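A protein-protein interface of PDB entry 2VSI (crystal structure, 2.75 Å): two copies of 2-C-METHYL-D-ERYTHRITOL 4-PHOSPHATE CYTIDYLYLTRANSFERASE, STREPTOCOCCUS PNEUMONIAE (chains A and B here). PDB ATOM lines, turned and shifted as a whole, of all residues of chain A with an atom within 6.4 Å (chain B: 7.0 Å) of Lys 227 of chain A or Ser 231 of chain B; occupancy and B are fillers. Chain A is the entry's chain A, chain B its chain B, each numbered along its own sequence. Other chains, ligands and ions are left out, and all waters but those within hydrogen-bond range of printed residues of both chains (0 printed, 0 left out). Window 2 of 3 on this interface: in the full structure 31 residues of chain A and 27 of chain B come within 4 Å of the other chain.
The backbone NH (N) of Thr 224 of chain A lies close to the side-chain hydroxyl (OG1) of Thr 222 of chain A (3.2 Å).
The side-chain hydroxyl (OG) of Ser 231 of chain A is in hydrogen-bond range of the backbone carbonyl oxygen (O) of Lys 227 of chain A (3.5 Å).
OG of Ser 231 of chain A sits at hydrogen-bond distance from O of Ile 228 of chain A (2.9 Å).
The side-chain hydroxyl (OG) of Ser 231 of chain B lies within hydrogen-bond range of the backbone carbonyl oxygen (O) of Ile 228 of chain B (2.6 Å).
OG of Ser 231 of chain B lies within hydrogen-bond range of NZ of Lys 227 of chain A, 3.3 Å away.
Lys 227 of chain A touches Ile 228 of chain B, but with the chains exchanged Ile 228 of chain A does not touch Lys 227 of chain B (7.2 Å).
Lys 227 of chain A touches Ser 231 of chain B, and with the chains exchanged Ser 231 of chain A touches Lys 227 of chain B.
Ile 228 of chain B touches its own counterpart, Ile 228 of chain A.
7 positions are printed for both chains.
Of the 12 printed residues of chain A, 4 touch a printed residue of chain B.
Hydrophobic or aromatic side chains of chain A within 4 Å of the printed part of chain B: Ile 228.
Printed residues of chain B that touch a printed residue of chain A: Lys 227, Ile 228, Ser 231 and Met 232.
Hydrophobic or aromatic side chains of chain B within 4 Å of the printed part of chain A: Ile 228 and Met 232.
Among the printed residues, no Asp or Glu carboxylate lies within 4 Å of a Lys or Arg side-chain nitrogen of the other chain.
Of chain B, only Ile 228 (3.7 Å) and Ser 231 (3.3 Å) come within 4 Å of Lys 227 of chain A.
Ser 231 of chain B touches one residue of chain A.
Of the printed residues of chain A, Met 232 of chain B touches Thr 224.
Printed residues of chain B within 4 Å of Ser 231 of chain A: Lys 227.
Of the printed residues of chain A, Lys 227 of chain B touches Ser 231 (3.9 Å).
Printed residues of chain A within 4 Å of Ile 228 of chain B: Thr 224 (3.9 Å), Lys 227 (3.7 Å) and Ile 228 (3.5 Å).
Met 232 of chain A touches none of the printed residues of chain B.
The nearest printed residue of chain A that does not touch Ser 231 of chain B is Thr 224 of chain A (7.2 Å).
Among the printed residues, pairs that only touch across the chains: Thr 224 of chain A with Ile 228 of chain B (3.9 Å), Thr 224 of chain A with Met 232 of chain B (3.7 Å), Lys 227 of chain A with Ile 228 of chain B (3.7 Å), Ile 228 of chain A with Ile 228 of chain B (3.5 Å) and Ser 231 of chain A with Lys 227 of chain B (3.9 Å).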
ATOM      1  N   ILE A 220       1.529  22.255  11.437  1.00  0.00           N
ATOM      2  CA  ILE A 220       0.977  23.604  11.429  1.00  0.00           C
ATOM      3  C   ILE A 220       1.934  24.585  10.755  1.00  0.00           C
ATOM      4  O   ILE A 220       2.835  25.134  11.398  1.00  0.00           O
ATOM      5  CB  ILE A 220       0.599  24.068  12.860  1.00  0.00           C
ATOM      6  CG1 ILE A 220      -0.152  22.950  13.601  1.00  0.00           C
ATOM      7  CG2 ILE A 220      -0.223  25.366  12.808  1.00  0.00           C
ATOM      8  CD1 ILE A 220      -0.610  23.306  15.004  1.00  0.00           C
ATOM      9  N   THR A 222       0.586  26.865   7.895  1.00  0.00           N
ATOM     10  CA  THR A 222      -0.179  28.001   7.394  1.00  0.00           C
ATOM     11  C   THR A 222      -1.210  28.494   8.402  1.00  0.00           C
ATOM     12  O   THR A 222      -1.563  27.781   9.336  1.00  0.00           O
ATOM     13  CB  THR A 222      -0.910  27.685   6.059  1.00  0.00           C
ATOM     14  OG1 THR A 222      -2.005  26.795   6.303  1.00  0.00           O
ATOM     15  CG2 THR A 222       0.039  27.072   5.022  1.00  0.00           C
ATOM     16  N   VAL A 223      -1.690  29.719   8.199  1.00  0.00           N
ATOM     17  CA  VAL A 223      -2.779  30.280   9.000  1.00  0.00           C
ATOM     18  C   VAL A 223      -4.067  29.438   8.900  1.00  0.00           C
ATOM     19  O   VAL A 223      -4.953  29.541   9.755  1.00  0.00           O
ATOM     20  CB  VAL A 223      -3.078  31.726   8.601  1.00  0.00           C
ATOM     21  CG1 VAL A 223      -3.688  32.473   9.774  1.00  0.00           C
ATOM     22  CG2 VAL A 223      -1.806  32.424   8.149  1.00  0.00           C
ATOM     23  N   THR A 224      -4.148  28.610   7.855  1.00  0.00           N
ATOM     24  CA  THR A 224      -5.232  27.637   7.679  1.00  0.00           C
ATOM     25  C   THR A 224      -5.026  26.456   8.615  1.00  0.00           C
ATOM     26  O   THR A 224      -5.966  26.020   9.277  1.00  0.00           O
ATOM     27  CB  THR A 224      -5.332  27.148   6.211  1.00  0.00           C
ATOM     28  OG1 THR A 224      -5.680  28.250   5.363  1.00  0.00           O
ATOM     29  CG2 THR A 224      -6.378  26.062   6.058  1.00  0.00           C
ATOM     30  N   ASP A 225      -3.795  25.949   8.671  1.00  0.00           N
ATOM     31  CA  ASP A 225      -3.422  24.898   9.617  1.00  0.00           C
ATOM     32  C   ASP A 225      -3.757  25.321  11.053  1.00  0.00           C
ATOM     33  O   ASP A 225      -4.228  24.512  11.847  1.00  0.00           O
ATOM     34  CB  ASP A 225      -1.934  24.559   9.508  1.00  0.00           C
ATOM     35  CG  ASP A 225      -1.531  24.046   8.132  1.00  0.00           C
ATOM     36  OD1 ASP A 225      -2.283  23.274   7.501  1.00  0.00           O
ATOM     37  OD2 ASP A 225      -0.427  24.401   7.684  1.00  0.00           O
ATOM     38  N   LEU A 226      -3.540  26.597  11.370  1.00  0.00           N
ATOM     39  CA  LEU A 226      -3.863  27.142  12.696  1.00  0.00           C
ATOM     40  C   LEU A 226      -5.335  26.949  13.055  1.00  0.00           C
ATOM     41  O   LEU A 226      -5.641  26.474  14.148  1.00  0.00           O
ATOM     42  CB  LEU A 226      -3.477  28.625  12.802  1.00  0.00           C
ATOM     43  CG  LEU A 226      -2.728  29.083  14.062  1.00  0.00           C
ATOM     44  CD1 LEU A 226      -2.817  30.596  14.202  1.00  0.00           C
ATOM     45  CD2 LEU A 226      -3.228  28.405  15.338  1.00  0.00           C
ATOM     46  N   LYS A 227      -6.229  27.310  12.134  1.00  0.00           N
ATOM     47  CA  LYS A 227      -7.675  27.142  12.325  1.00  0.00           C
ATOM     48  C   LYS A 227      -8.067  25.679  12.575  1.00  0.00           C
ATOM     49  O   LYS A 227      -8.841  25.390  13.496  1.00  0.00           O
ATOM     50  CB  LYS A 227      -8.454  27.663  11.118  1.00  0.00           C
ATOM     51  CG  LYS A 227      -8.184  29.099  10.718  1.00  0.00           C
ATOM     52  CD  LYS A 227      -8.813  29.386   9.353  1.00  0.00           C
ATOM     53  CE  LYS A 227      -8.330  30.704   8.763  1.00  0.00           C
ATOM     54  NZ  LYS A 227      -8.833  30.873   7.371  1.00  0.00           N
ATOM     55  N   ILE A 228      -7.537  24.765  11.755  1.00  0.00           N
ATOM     56  CA  ILE A 228      -7.829  23.337  11.895  1.00  0.00           C
ATOM     57  C   ILE A 228      -7.441  22.855  13.287  1.00  0.00           C
ATOM     58  O   ILE A 228      -8.179  22.087  13.913  1.00  0.00           O
ATOM     59  CB  ILE A 228      -7.152  22.481  10.790  1.00  0.00           C
ATOM     60  CG1 ILE A 228      -7.886  22.663   9.457  1.00  0.00           C
ATOM     61  CG2 ILE A 228      -7.139  20.995  11.170  1.00  0.00           C
ATOM     62  CD1 ILE A 228      -7.216  22.003   8.265  1.00  0.00           C
ATOM     63  N   ALA A 229      -6.295  23.333  13.768  1.00  0.00           N
ATOM     64  CA  ALA A 229      -5.798  22.995  15.095  1.00  0.00           C
ATOM     65  C   ALA A 229      -6.713  23.513  16.202  1.00  0.00           C
ATOM     66  O   ALA A 229      -7.065  22.769  17.119  1.00  0.00           O
ATOM     67  CB  ALA A 229      -4.395  23.532  15.280  1.00  0.00           C
ATOM     68  N   LYS A 230      -7.090  24.787  16.112  1.00  0.00           N
ATOM     69  CA  LYS A 230      -8.000  25.407  17.076  1.00  0.00           C
ATOM     70  C   LYS A 230      -9.305  24.625  17.247  1.00  0.00           C
ATOM     71  O   LYS A 230      -9.729  24.363  18.374  1.00  0.00           O
ATOM     72  CB  LYS A 230      -8.310  26.850  16.675  1.00  0.00           C
ATOM     73  CG  LYS A 230      -7.167  27.827  16.888  1.00  0.00           C
ATOM     74  CD  LYS A 230      -7.632  29.222  16.557  1.00  0.00           C
ATOM     75  CE  LYS A 230      -6.609  30.267  16.908  1.00  0.00           C
ATOM     76  NZ  LYS A 230      -7.270  31.602  16.814  1.00  0.00           N
ATOM     77  N   SER A 231      -9.925  24.248  16.127  1.00  0.00           N
ATOM     78  CA  SER A 231     -11.151  23.446  16.138  1.00  0.00           C
ATOM     79  C   SER A 231     -10.936  22.034  16.695  1.00  0.00           C
ATOM     80  O   SER A 231     -11.890  21.369  17.086  1.00  0.00           O
ATOM     81  CB  SER A 231     -11.787  23.387  14.742  1.00  0.00           C
ATOM     82  OG  SER A 231     -10.967  22.685  13.823  1.00  0.00           O
ATOM     83  N   MET A 232      -9.685  21.583  16.737  1.00  0.00           N
ATOM     84  CA  MET A 232      -9.363  20.280  17.323  1.00  0.00           C
ATOM     85  C   MET A 232      -9.212  20.320  18.846  1.00  0.00           C
ATOM     86  O   MET A 232      -9.145  19.274  19.481  1.00  0.00           O
ATOM     87  CB  MET A 232      -8.107  19.677  16.681  1.00  0.00           C
ATOM     88  CG  MET A 232      -8.333  19.054  15.316  1.00  0.00           C
ATOM     89  SD  MET A 232      -6.806  18.719  14.419  1.00  0.00           S
ATOM     90  CE  MET A 232      -6.251  17.222  15.230  1.00  0.00           C
ATOM     91  N   LEU B  28     -23.131  28.068   2.487  1.00  0.00           N
ATOM     92  CA  LEU B  28     -21.827  28.670   2.710  1.00  0.00           C
ATOM     93  C   LEU B  28     -22.066  30.175   2.718  1.00  0.00           C
ATOM     94  O   LEU B  28     -22.350  30.768   1.676  1.00  0.00           O
ATOM     95  CB  LEU B  28     -20.874  28.299   1.569  1.00  0.00           C
ATOM     96  CG  LEU B  28     -19.341  28.247   1.682  1.00  0.00           C
ATOM     97  CD1 LEU B  28     -18.712  28.965   0.493  1.00  0.00           C
ATOM     98  CD2 LEU B  28     -18.774  28.766   2.994  1.00  0.00           C
ATOM     99  N   PHE B 118     -13.806  28.171  -4.413  1.00  0.00           N
ATOM    100  CA  PHE B 118     -12.804  29.252  -4.336  1.00  0.00           C
ATOM    101  C   PHE B 118     -11.885  29.303  -5.553  1.00  0.00           C
ATOM    102  O   PHE B 118     -10.713  29.670  -5.466  1.00  0.00           O
ATOM    103  CB  PHE B 118     -12.004  29.173  -3.028  1.00  0.00           C
ATOM    104  CG  PHE B 118     -12.861  29.257  -1.800  1.00  0.00           C
ATOM    105  CD1 PHE B 118     -13.354  30.482  -1.363  1.00  0.00           C
ATOM    106  CD2 PHE B 118     -13.192  28.108  -1.090  1.00  0.00           C
ATOM    107  CE1 PHE B 118     -14.161  30.567  -0.228  1.00  0.00           C
ATOM    108  CE2 PHE B 118     -13.993  28.179   0.047  1.00  0.00           C
ATOM    109  CZ  PHE B 118     -14.479  29.414   0.479  1.00  0.00           C
ATOM    110  N   LEU B 226     -15.663  22.399   5.865  1.00  0.00           N
ATOM    111  CA  LEU B 226     -16.763  23.356   5.821  1.00  0.00           C
ATOM    112  C   LEU B 226     -16.484  24.497   6.796  1.00  0.00           C
ATOM    113  O   LEU B 226     -16.752  25.658   6.481  1.00  0.00           O
ATOM    114  CB  LEU B 226     -18.097  22.680   6.157  1.00  0.00           C
ATOM    115  CG  LEU B 226     -19.336  22.949   5.288  1.00  0.00           C
ATOM    116  CD1 LEU B 226     -20.603  22.856   6.131  1.00  0.00           C
ATOM    117  CD2 LEU B 226     -19.304  24.292   4.549  1.00  0.00           C
ATOM    118  N   LYS B 227     -15.932  24.161   7.967  1.00  0.00           N
ATOM    119  CA  LYS B 227     -15.543  25.158   8.969  1.00  0.00           C
ATOM    120  C   LYS B 227     -14.460  26.115   8.442  1.00  0.00           C
ATOM    121  O   LYS B 227     -14.564  27.334   8.612  1.00  0.00           O
ATOM    122  CB  LYS B 227     -15.106  24.492  10.283  1.00  0.00           C
ATOM    123  CG  LYS B 227     -14.776  25.470  11.416  1.00  0.00           C
ATOM    124  CD  LYS B 227     -14.870  24.813  12.791  1.00  0.00           C
ATOM    125  CE  LYS B 227     -14.749  25.847  13.914  1.00  0.00           C
ATOM    126  NZ  LYS B 227     -15.577  25.495  15.114  1.00  0.00           N
ATOM    127  N   ILE B 228     -13.435  25.570   7.792  1.00  0.00           N
ATOM    128  CA  ILE B 228     -12.424  26.409   7.157  1.00  0.00           C
ATOM    129  C   ILE B 228     -13.078  27.312   6.110  1.00  0.00           C
ATOM    130  O   ILE B 228     -12.815  28.515   6.064  1.00  0.00           O
ATOM    131  CB  ILE B 228     -11.290  25.574   6.504  1.00  0.00           C
ATOM    132  CG1 ILE B 228     -10.612  24.649   7.525  1.00  0.00           C
ATOM    133  CG2 ILE B 228     -10.265  26.478   5.815  1.00  0.00           C
ATOM    134  CD1 ILE B 228      -9.979  25.356   8.715  1.00  0.00           C
ATOM    135  N   ALA B 229     -13.944  26.723   5.290  1.00  0.00           N
ATOM    136  CA  ALA B 229     -14.601  27.434   4.201  1.00  0.00           C
ATOM    137  C   ALA B 229     -15.436  28.624   4.680  1.00  0.00           C
ATOM    138  O   ALA B 229     -15.350  29.714   4.113  1.00  0.00           O
ATOM    139  CB  ALA B 229     -15.452  26.473   3.388  1.00  0.00           C
ATOM    140  N   LYS B 230     -16.236  28.408   5.725  1.00  0.00           N
ATOM    141  CA  LYS B 230     -17.071  29.457   6.312  1.00  0.00           C
ATOM    142  C   LYS B 230     -16.255  30.660   6.802  1.00  0.00           C
ATOM    143  O   LYS B 230     -16.692  31.808   6.671  1.00  0.00           O
ATOM    144  CB  LYS B 230     -17.947  28.888   7.435  1.00  0.00           C
ATOM    145  CG  LYS B 230     -19.228  28.205   6.941  1.00  0.00           C
ATOM    146  CD  LYS B 230     -20.148  27.780   8.094  1.00  0.00           C
ATOM    147  CE  LYS B 230     -21.514  27.282   7.589  1.00  0.00           C
ATOM    148  NZ  LYS B 230     -22.435  28.377   7.119  1.00  0.00           N
ATOM    149  N   SER B 231     -15.068  30.391   7.349  1.00  0.00           N
ATOM    150  CA  SER B 231     -14.156  31.443   7.801  1.00  0.00           C
ATOM    151  C   SER B 231     -13.512  32.198   6.636  1.00  0.00           C
ATOM    152  O   SER B 231     -13.102  33.350   6.786  1.00  0.00           O
ATOM    153  CB  SER B 231     -13.063  30.859   8.698  1.00  0.00           C
ATOM    154  OG  SER B 231     -12.069  30.211   7.926  1.00  0.00           O
ATOM    155  N   MET B 232     -13.416  31.542   5.482  1.00  0.00           N
ATOM    156  CA  MET B 232     -12.780  32.135   4.310  1.00  0.00           C
ATOM    157  C   MET B 232     -13.661  33.155   3.580  1.00  0.00           C
ATOM    158  O   MET B 232     -13.152  34.011   2.860  1.00  0.00           O
ATOM    159  CB  MET B 232     -12.276  31.042   3.359  1.00  0.00           C
ATOM    160  CG  MET B 232     -10.891  30.518   3.724  1.00  0.00           C
ATOM    161  SD  MET B 232     -10.345  29.090   2.755  1.00  0.00           S
ATOM    162  CE  MET B 232      -8.611  28.976   3.207  1.00  0.00           C
ATOM    163  N   ILE B 233     -14.974  33.067   3.781  1.00  0.00           N
ATOM    164  CA  ILE B 233     -15.927  33.968   3.130  1.00  0.00           C
ATOM    165  C   ILE B 233     -16.762  34.719   4.173  1.00  0.00           C
ATOM    166  O   ILE B 233     -17.062  35.902   4.012  1.00  0.00           O
ATOM    167  CB  ILE B 233     -16.855  33.198   2.133  1.00  0.00           C
ATOM    168  CG1 ILE B 233     -17.511  34.149   1.115  1.00  0.00           C
ATOM    169  CG2 ILE B 233     -17.898  32.363   2.877  1.00  0.00           C
ATOM    170  CD1 ILE B 233     -16.719  34.340  -0.190  1.00  0.00           C
